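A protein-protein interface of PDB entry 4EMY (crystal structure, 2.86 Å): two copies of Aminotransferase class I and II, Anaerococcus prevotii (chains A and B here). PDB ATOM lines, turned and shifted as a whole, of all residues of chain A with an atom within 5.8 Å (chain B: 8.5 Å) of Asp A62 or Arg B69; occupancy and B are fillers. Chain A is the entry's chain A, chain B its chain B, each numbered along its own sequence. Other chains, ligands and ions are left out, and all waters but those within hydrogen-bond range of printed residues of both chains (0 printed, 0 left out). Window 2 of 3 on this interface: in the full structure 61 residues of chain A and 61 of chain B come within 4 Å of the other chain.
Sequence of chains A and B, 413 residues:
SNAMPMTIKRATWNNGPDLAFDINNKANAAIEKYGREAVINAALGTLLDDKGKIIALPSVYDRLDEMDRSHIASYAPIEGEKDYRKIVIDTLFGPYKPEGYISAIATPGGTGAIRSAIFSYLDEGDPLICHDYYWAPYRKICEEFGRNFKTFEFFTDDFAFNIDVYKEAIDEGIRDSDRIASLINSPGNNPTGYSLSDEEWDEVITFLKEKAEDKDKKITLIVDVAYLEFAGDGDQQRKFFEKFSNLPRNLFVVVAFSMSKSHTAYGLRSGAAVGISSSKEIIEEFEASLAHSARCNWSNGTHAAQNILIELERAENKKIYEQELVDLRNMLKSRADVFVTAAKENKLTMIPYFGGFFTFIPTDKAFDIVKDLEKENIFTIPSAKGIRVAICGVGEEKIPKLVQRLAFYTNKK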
ATOM      1  N   ILE A  54       1.848   6.459  34.273  1.00  0.00           N
ATOM      2  CA  ILE A  54       2.620   7.406  33.474  1.00  0.00           C
ATOM      3  C   ILE A  54       2.012   8.816  33.466  1.00  0.00           C
ATOM      4  O   ILE A  54       0.808   8.991  33.690  1.00  0.00           O
ATOM      5  CB  ILE A  54       2.792   6.885  32.033  1.00  0.00           C
ATOM      6  CG1 ILE A  54       3.999   7.547  31.360  1.00  0.00           C
ATOM      7  CG2 ILE A  54       1.503   7.071  31.242  1.00  0.00           C
ATOM      8  CD1 ILE A  54       4.417   6.900  30.062  1.00  0.00           C
ATOM      9  N   ALA A  56       1.334  11.870  31.045  1.00  0.00           N
ATOM     10  CA  ALA A  56       1.263  12.457  29.717  1.00  0.00           C
ATOM     11  C   ALA A  56       0.699  13.867  29.856  1.00  0.00           C
ATOM     12  O   ALA A  56      -0.494  14.051  30.149  1.00  0.00           O
ATOM     13  CB  ALA A  56       0.407  11.604  28.793  1.00  0.00           C
ATOM     14  N   LEU A  57       1.574  14.856  29.679  1.00  0.00           N
ATOM     15  CA  LEU A  57       1.205  16.264  29.821  1.00  0.00           C
ATOM     16  C   LEU A  57       0.066  16.644  28.873  1.00  0.00           C
ATOM     17  O   LEU A  57       0.197  16.496  27.658  1.00  0.00           O
ATOM     18  CB  LEU A  57       2.419  17.155  29.567  1.00  0.00           C
ATOM     19  CG  LEU A  57       3.535  17.111  30.605  1.00  0.00           C
ATOM     20  CD1 LEU A  57       4.810  17.686  30.018  1.00  0.00           C
ATOM     21  CD2 LEU A  57       3.134  17.858  31.867  1.00  0.00           C
ATOM     22  N   PRO A  58      -1.067  17.114  29.421  1.00  0.00           N
ATOM     23  CA  PRO A  58      -2.183  17.512  28.564  1.00  0.00           C
ATOM     24  C   PRO A  58      -1.797  18.554  27.507  1.00  0.00           C
ATOM     25  O   PRO A  58      -2.232  18.451  26.365  1.00  0.00           O
ATOM     26  CB  PRO A  58      -3.191  18.096  29.559  1.00  0.00           C
ATOM     27  CG  PRO A  58      -2.904  17.374  30.825  1.00  0.00           C
ATOM     28  CD  PRO A  58      -1.413  17.214  30.849  1.00  0.00           C
ATOM     29  N   SER A  59      -0.972  19.529  27.885  1.00  0.00           N
ATOM     30  CA  SER A  59      -0.548  20.595  26.978  1.00  0.00           C
ATOM     31  C   SER A  59       0.195  20.058  25.761  1.00  0.00           C
ATOM     32  O   SER A  59       0.162  20.671  24.698  1.00  0.00           O
ATOM     33  CB  SER A  59       0.333  21.599  27.708  1.00  0.00           C
ATOM     34  OG  SER A  59       1.501  20.964  28.192  1.00  0.00           O
ATOM     35  N   VAL A  60       0.866  18.920  25.925  1.00  0.00           N
ATOM     36  CA  VAL A  60       1.492  18.218  24.811  1.00  0.00           C
ATOM     37  C   VAL A  60       0.448  17.443  23.996  1.00  0.00           C
ATOM     38  O   VAL A  60       0.243  17.727  22.819  1.00  0.00           O
ATOM     39  CB  VAL A  60       2.629  17.284  25.287  1.00  0.00           C
ATOM     40  CG1 VAL A  60       3.254  16.543  24.112  1.00  0.00           C
ATOM     41  CG2 VAL A  60       3.696  18.072  26.028  1.00  0.00           C
ATOM     42  N   TYR A  61      -0.228  16.489  24.629  1.00  0.00           N
ATOM     43  CA  TYR A  61      -1.159  15.591  23.921  1.00  0.00           C
ATOM     44  C   TYR A  61      -2.495  16.191  23.446  1.00  0.00           C
ATOM     45  O   TYR A  61      -3.159  15.601  22.586  1.00  0.00           O
ATOM     46  CB  TYR A  61      -1.352  14.284  24.703  1.00  0.00           C
ATOM     47  CG  TYR A  61      -0.074  13.490  24.727  1.00  0.00           C
ATOM     48  CD1 TYR A  61       0.190  12.533  23.753  1.00  0.00           C
ATOM     49  CD2 TYR A  61       0.907  13.747  25.686  1.00  0.00           C
ATOM     50  CE1 TYR A  61       1.382  11.835  23.753  1.00  0.00           C
ATOM     51  CE2 TYR A  61       2.105  13.055  25.691  1.00  0.00           C
ATOM     52  CZ  TYR A  61       2.335  12.101  24.725  1.00  0.00           C
ATOM     53  OH  TYR A  61       3.522  11.412  24.733  1.00  0.00           O
ATOM     54  N   ASP A  62      -2.872  17.359  23.968  1.00  0.00           N
ATOM     55  CA  ASP A  62      -4.008  18.098  23.418  1.00  0.00           C
ATOM     56  C   ASP A  62      -3.717  18.555  21.986  1.00  0.00           C
ATOM     57  O   ASP A  62      -4.602  18.524  21.127  1.00  0.00           O
ATOM     58  CB  ASP A  62      -4.386  19.304  24.289  1.00  0.00           C
ATOM     59  CG  ASP A  62      -5.070  18.910  25.592  1.00  0.00           C
ATOM     60  OD1 ASP A  62      -5.715  17.841  25.643  1.00  0.00           O
ATOM     61  OD2 ASP A  62      -4.960  19.681  26.569  1.00  0.00           O
ATOM     62  N   ARG A  63      -2.481  18.975  21.734  1.00  0.00           N
ATOM     63  CA  ARG A  63      -2.074  19.412  20.397  1.00  0.00           C
ATOM     64  C   ARG A  63      -2.219  18.299  19.370  1.00  0.00           C
ATOM     65  O   ARG A  63      -2.716  18.531  18.272  1.00  0.00           O
ATOM     66  CB  ARG A  63      -0.634  19.933  20.397  1.00  0.00           C
ATOM     67  CG  ARG A  63      -0.362  21.020  21.422  1.00  0.00           C
ATOM     68  CD  ARG A  63      -1.319  22.191  21.307  1.00  0.00           C
ATOM     69  NE  ARG A  63      -1.693  22.651  22.642  1.00  0.00           N
ATOM     70  CZ  ARG A  63      -2.914  22.570  23.164  1.00  0.00           C
ATOM     71  NH1 ARG A  63      -3.919  22.070  22.461  1.00  0.00           N
ATOM     72  NH2 ARG A  63      -3.132  23.011  24.395  1.00  0.00           N
ATOM     73  N   LEU A  64      -1.779  17.095  19.732  1.00  0.00           N
ATOM     74  CA  LEU A  64      -1.959  15.912  18.892  1.00  0.00           C
ATOM     75  C   LEU A  64      -3.446  15.641  18.662  1.00  0.00           C
ATOM     76  O   LEU A  64      -3.858  15.342  17.544  1.00  0.00           O
ATOM     77  CB  LEU A  64      -1.267  14.695  19.519  1.00  0.00           C
ATOM     78  CG  LEU A  64      -1.433  13.328  18.848  1.00  0.00           C
ATOM     79  CD1 LEU A  64      -0.752  13.285  17.488  1.00  0.00           C
ATOM     80  CD2 LEU A  64      -0.921  12.214  19.747  1.00  0.00           C
ATOM     81  N   ASP A  65      -4.241  15.764  19.722  1.00  0.00           N
ATOM     82  CA  ASP A  65      -5.694  15.602  19.625  1.00  0.00           C
ATOM     83  C   ASP A  65      -6.329  16.563  18.610  1.00  0.00           C
ATOM     84  O   ASP A  65      -7.212  16.168  17.848  1.00  0.00           O
ATOM     85  CB  ASP A  65      -6.362  15.762  21.004  1.00  0.00           C
ATOM     86  CG  ASP A  65      -6.351  14.473  21.827  1.00  0.00           C
ATOM     87  OD1 ASP A  65      -6.365  13.377  21.227  1.00  0.00           O
ATOM     88  OD2 ASP A  65      -6.348  14.555  23.080  1.00  0.00           O
ATOM     89  N   GLU A  66      -5.861  17.810  18.595  1.00  0.00           N
ATOM     90  CA  GLU A  66      -6.471  18.866  17.781  1.00  0.00           C
ATOM     91  C   GLU A  66      -5.851  18.996  16.402  1.00  0.00           C
ATOM     92  O   GLU A  66      -6.412  19.641  15.519  1.00  0.00           O
ATOM     93  CB  GLU A  66      -6.382  20.203  18.503  1.00  0.00           C
ATOM     94  CG  GLU A  66      -7.320  20.312  19.694  1.00  0.00           C
ATOM     95  CD  GLU A  66      -6.804  21.263  20.759  1.00  0.00           C
ATOM     96  OE1 GLU A  66      -5.644  21.732  20.639  1.00  0.00           O
ATOM     97  OE2 GLU A  66      -7.560  21.538  21.718  1.00  0.00           O
ATOM     98  N   MET A  67      -4.695  18.368  16.228  1.00  0.00           N
ATOM     99  CA  MET A  67      -3.932  18.417  14.986  1.00  0.00           C
ATOM    100  C   MET A  67      -4.689  17.813  13.813  1.00  0.00           C
ATOM    101  O   MET A  67      -5.367  16.794  13.960  1.00  0.00           O
ATOM    102  CB  MET A  67      -2.617  17.664  15.171  1.00  0.00           C
ATOM    103  CG  MET A  67      -1.642  17.850  14.067  1.00  0.00           C
ATOM    104  SD  MET A  67       0.077  17.232  14.673  1.00  0.00           S
ATOM    105  CE  MET A  67       0.414  18.558  16.070  1.00  0.00           C
ATOM    106  N   LEU B  64      -6.218   6.162  16.799  1.00  0.00           N
ATOM    107  CA  LEU B  64      -5.309   7.066  17.493  1.00  0.00           C
ATOM    108  C   LEU B  64      -6.071   8.044  18.391  1.00  0.00           C
ATOM    109  O   LEU B  64      -5.677   8.268  19.536  1.00  0.00           O
ATOM    110  CB  LEU B  64      -4.402   7.805  16.505  1.00  0.00           C
ATOM    111  CG  LEU B  64      -3.417   8.817  17.094  1.00  0.00           C
ATOM    112  CD1 LEU B  64      -2.360   8.134  17.945  1.00  0.00           C
ATOM    113  CD2 LEU B  64      -2.770   9.615  15.982  1.00  0.00           C
ATOM    114  N   ASP B  65      -7.166   8.603  17.870  1.00  0.00           N
ATOM    115  CA  ASP B  65      -8.051   9.500  18.634  1.00  0.00           C
ATOM    116  C   ASP B  65      -8.605   8.840  19.895  1.00  0.00           C
ATOM    117  O   ASP B  65      -8.698   9.469  20.950  1.00  0.00           O
ATOM    118  CB  ASP B  65      -9.220   9.978  17.762  1.00  0.00           C
ATOM    119  CG  ASP B  65      -8.788  10.931  16.655  1.00  0.00           C
ATOM    120  OD1 ASP B  65      -7.861  11.745  16.877  1.00  0.00           O
ATOM    121  OD2 ASP B  65      -9.396  10.873  15.560  1.00  0.00           O
ATOM    122  N   GLU B  66      -8.957   7.565  19.759  1.00  0.00           N
ATOM    123  CA  GLU B  66      -9.583   6.774  20.813  1.00  0.00           C
ATOM    124  C   GLU B  66      -8.582   6.203  21.808  1.00  0.00           C
ATOM    125  O   GLU B  66      -8.942   5.828  22.923  1.00  0.00           O
ATOM    126  CB  GLU B  66     -10.358   5.622  20.181  1.00  0.00           C
ATOM    127  CG  GLU B  66     -11.618   6.043  19.439  1.00  0.00           C
ATOM    128  CD  GLU B  66     -12.266   4.888  18.694  1.00  0.00           C
ATOM    129  OE1 GLU B  66     -11.662   3.790  18.655  1.00  0.00           O
ATOM    130  OE2 GLU B  66     -13.373   5.079  18.141  1.00  0.00           O
ATOM    131  N   MET B  67      -7.325   6.139  21.385  1.00  0.00           N
ATOM    132  CA  MET B  67      -6.262   5.486  22.140  1.00  0.00           C
ATOM    133  C   MET B  67      -5.946   6.199  23.445  1.00  0.00           C
ATOM    134  O   MET B  67      -5.934   7.431  23.513  1.00  0.00           O
ATOM    135  CB  MET B  67      -5.004   5.405  21.284  1.00  0.00           C
ATOM    136  CG  MET B  67      -3.945   4.473  21.808  1.00  0.00           C
ATOM    137  SD  MET B  67      -2.553   4.247  20.475  1.00  0.00           S
ATOM    138  CE  MET B  67      -3.609   3.247  19.162  1.00  0.00           C
ATOM    139  N   ASP B  68      -5.682   5.398  24.473  1.00  0.00           N
ATOM    140  CA  ASP B  68      -5.261   5.884  25.776  1.00  0.00           C
ATOM    141  C   ASP B  68      -3.952   6.653  25.668  1.00  0.00           C
ATOM    142  O   ASP B  68      -3.002   6.186  25.031  1.00  0.00           O
ATOM    143  CB  ASP B  68      -5.077   4.697  26.712  1.00  0.00           C
ATOM    144  CG  ASP B  68      -5.385   5.036  28.145  1.00  0.00           C
ATOM    145  OD1 ASP B  68      -4.942   6.107  28.631  1.00  0.00           O
ATOM    146  OD2 ASP B  68      -6.072   4.216  28.792  1.00  0.00           O
ATOM    147  N   ARG B  69      -3.909   7.831  26.290  1.00  0.00           N
ATOM    148  CA  ARG B  69      -2.717   8.685  26.275  1.00  0.00           C
ATOM    149  C   ARG B  69      -1.434   7.907  26.541  1.00  0.00           C
ATOM    150  O   ARG B  69      -0.407   8.172  25.919  1.00  0.00           O
ATOM    151  CB  ARG B  69      -2.848   9.826  27.291  1.00  0.00           C
ATOM    152  CG  ARG B  69      -2.830  11.227  26.696  1.00  0.00           C
ATOM    153  CD  ARG B  69      -4.204  11.636  26.212  1.00  0.00           C
ATOM    154  NE  ARG B  69      -4.237  12.994  25.681  1.00  0.00           N
ATOM    155  CZ  ARG B  69      -4.519  14.081  26.392  1.00  0.00           C
ATOM    156  NH1 ARG B  69      -4.786  13.994  27.688  1.00  0.00           N
ATOM    157  NH2 ARG B  69      -4.534  15.268  25.804  1.00  0.00           N
ATOM    158  N   SER B  70      -1.514   6.945  27.458  1.00  0.00           N
ATOM    159  CA  SER B  70      -0.368   6.142  27.879  1.00  0.00           C
ATOM    160  C   SER B  70       0.180   5.263  26.761  1.00  0.00           C
ATOM    161  O   SER B  70       1.379   4.983  26.719  1.00  0.00           O
ATOM    162  CB  SER B  70      -0.753   5.265  29.058  1.00  0.00           C
ATOM    163  OG  SER B  70      -1.888   4.490  28.724  1.00  0.00           O
ATOM    164  N   HIS B  71      -0.694   4.828  25.860  1.00  0.00           N
ATOM    165  CA  HIS B  71      -0.279   4.001  24.726  1.00  0.00           C
ATOM    166  C   HIS B  71       0.387   4.787  23.625  1.00  0.00           C
ATOM    167  O   HIS B  71       0.857   4.223  22.634  1.00  0.00           O
ATOM    168  CB  HIS B  71      -1.459   3.193  24.207  1.00  0.00           C
ATOM    169  CG  HIS B  71      -1.891   2.116  25.156  1.00  0.00           C
ATOM    170  ND1 HIS B  71      -2.742   2.351  26.174  1.00  0.00           N
ATOM    171  CD2 HIS B  71      -1.521   0.777  25.250  1.00  0.00           C
ATOM    172  CE1 HIS B  71      -2.927   1.216  26.874  1.00  0.00           C
ATOM    173  NE2 HIS B  71      -2.177   0.252  26.308  1.00  0.00           N
ATOM    174  N   ILE B  72       0.433   6.101  23.802  1.00  0.00           N
ATOM    175  CA  ILE B  72       1.154   6.977  22.902  1.00  0.00           C
ATOM    176  C   ILE B  72       2.445   7.426  23.610  1.00  0.00           C
ATOM    177  O   ILE B  72       3.534   7.405  23.030  1.00  0.00           O
ATOM    178  CB  ILE B  72       0.284   8.186  22.486  1.00  0.00           C
ATOM    179  CG1 ILE B  72      -1.061   7.708  21.920  1.00  0.00           C
ATOM    180  CG2 ILE B  72       1.019   9.056  21.476  1.00  0.00           C
ATOM    181  CD1 ILE B  72      -2.111   8.791  21.765  1.00  0.00           C
ATOM    182  N   ALA B  73       2.311   7.795  24.880  1.00  0.00           N
ATOM    183  CA  ALA B  73       3.415   8.359  25.640  1.00  0.00           C
ATOM    184  C   ALA B  73       4.533   7.372  25.976  1.00  0.00           C
ATOM    185  O   ALA B  73       5.702   7.695  25.805  1.00  0.00           O
ATOM    186  CB  ALA B  73       2.892   9.022  26.905  1.00  0.00           C
ATOM    187  N   SER B  74       4.180   6.186  26.469  1.00  0.00           N
ATOM    188  CA  SER B  74       5.171   5.238  27.003  1.00  0.00           C
ATOM    189  C   SER B  74       6.097   4.678  25.927  1.00  0.00           C
ATOM    190  O   SER B  74       5.747   4.670  24.750  1.00  0.00           O
ATOM    191  CB  SER B  74       4.471   4.088  27.733  1.00  0.00           C
ATOM    192  OG  SER B  74       3.638   3.347  26.860  1.00  0.00           O
ATOM    193  N   HIS B 303       5.322   4.000  19.370  1.00  0.00           N
ATOM    194  CA  HIS B 303       4.438   3.129  20.143  1.00  0.00           C
ATOM    195  C   HIS B 303       2.987   3.190  19.715  1.00  0.00           C
ATOM    196  O   HIS B 303       2.331   2.149  19.595  1.00  0.00           O
ATOM    197  CB  HIS B 303       4.602   3.422  21.628  1.00  0.00           C
ATOM    198  CG  HIS B 303       4.158   2.295  22.526  1.00  0.00           C
ATOM    199  ND1 HIS B 303       3.995   2.452  23.854  1.00  0.00           N
ATOM    200  CD2 HIS B 303       3.832   0.970  22.244  1.00  0.00           C
ATOM    201  CE1 HIS B 303       3.596   1.287  24.395  1.00  0.00           C
ATOM    202  NE2 HIS B 303       3.493   0.382  23.408  1.00  0.00           N
ATOM    203  N   ALA B 304       2.490   4.404  19.456  1.00  0.00           N
ATOM    204  CA  ALA B 304       1.114   4.626  18.998  1.00  0.00           C
ATOM    205  C   ALA B 304       0.793   3.800  17.765  1.00  0.00           C
ATOM    206  O   ALA B 304      -0.265   3.165  17.687  1.00  0.00           O
ATOM    207  CB  ALA B 304       0.883   6.102  18.710  1.00  0.00           C
ATOM    208  N   ASN B 307       0.434   0.047  18.440  1.00  0.00           N
ATOM    209  CA  ASN B 307      -0.872  -0.143  19.052  1.00  0.00           C
ATOM    210  C   ASN B 307      -2.034  -0.007  18.072  1.00  0.00           C
ATOM    211  O   ASN B 307      -3.025  -0.732  18.188  1.00  0.00           O
ATOM    212  CB  ASN B 307      -1.040   0.787  20.251  1.00  0.00           C
ATOM    213  CG  ASN B 307      -0.172   0.374  21.430  1.00  0.00           C
ATOM    214  OD1 ASN B 307      -0.061  -0.812  21.752  1.00  0.00           O
ATOM    215  ND2 ASN B 307       0.449   1.354  22.082  1.00  0.00           N
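Hydrophobic or aromatic side chains of chain B that line the printed part of chain A: Ile B72 and Ala B73. Of the 13 printed residues of chain A, 6 touch a printed residue of chain B. Hydrophobic or aromatic side chains of chain A within 4 Å of the printed part of chain B: Ile A54, Ala A56 and Tyr A61. Along chain A the printed residues that touch a printed residue of chain B span positions 54 to 65.
Of chain B, only Arg B69 (2.8 Å) comes within 4 Å of Asp A62. Of chain A, only Ala A56 (3.9 Å), Pro A58 (3.97 Å), Tyr A61 (3.3 Å), Asp A62 (2.8 Å) and Asp A65 (3.3 Å) come within 4 Å of Arg B69. Printed residues of chain B within 4 Å of Tyr A61: Arg B69 (3.3 Å), Ile B72 (3.6 Å) and Ala B73 (3.2 Å). Printed residues of chain B within 4 Å of Pro A58: Arg B69 (3.97 Å). Printed residues of chain A within 4 Å of Ser B74: Ile A54. Met A67 touches none of the printed residues of chain B. The nearest printed residue of chain B that does not touch Asp A62 is Asp B65 (8.6 Å). The nearest printed residue of chain B that does not touch Asp A65 is Asp B65 (4.6 Å).
The side-chain hydroxyl of Ser B70 is in hydrogen-bond range of a ring nitrogen (ND1) of His B71, 3.4 Å away. O of Ser B70 is in hydrogen-bond range of OG of Ser B74, 2.8 Å away. OD1 of Asp B68 sits at hydrogen-bond distance from OG of Ser B70. A ring nitrogen (ND1) of His B303 lies within hydrogen-bond range of the backbone carbonyl oxygen (O) of Ser B74.
Positions printed for both chains: 64, 65, 66 and 67.
Among the printed residues, pairs that only touch across the chains: Tyr A61 with Ala B73, Tyr A61 with Arg B69, Ile A54 with Ser B74, Tyr A61 with Ile B72, Ile A54 with Ser B70, Ala A56 with Arg B69 and Pro A58 with Arg B69.
The guanidinium group (NH2) of Arg B69 is in salt-bridge range of the side-chain carboxylate (OD1) of Asp A62, 2.8 Å away. OD2 of Asp A65 lies within salt-bridge range of NH2 of Arg B69 (3.3 Å).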
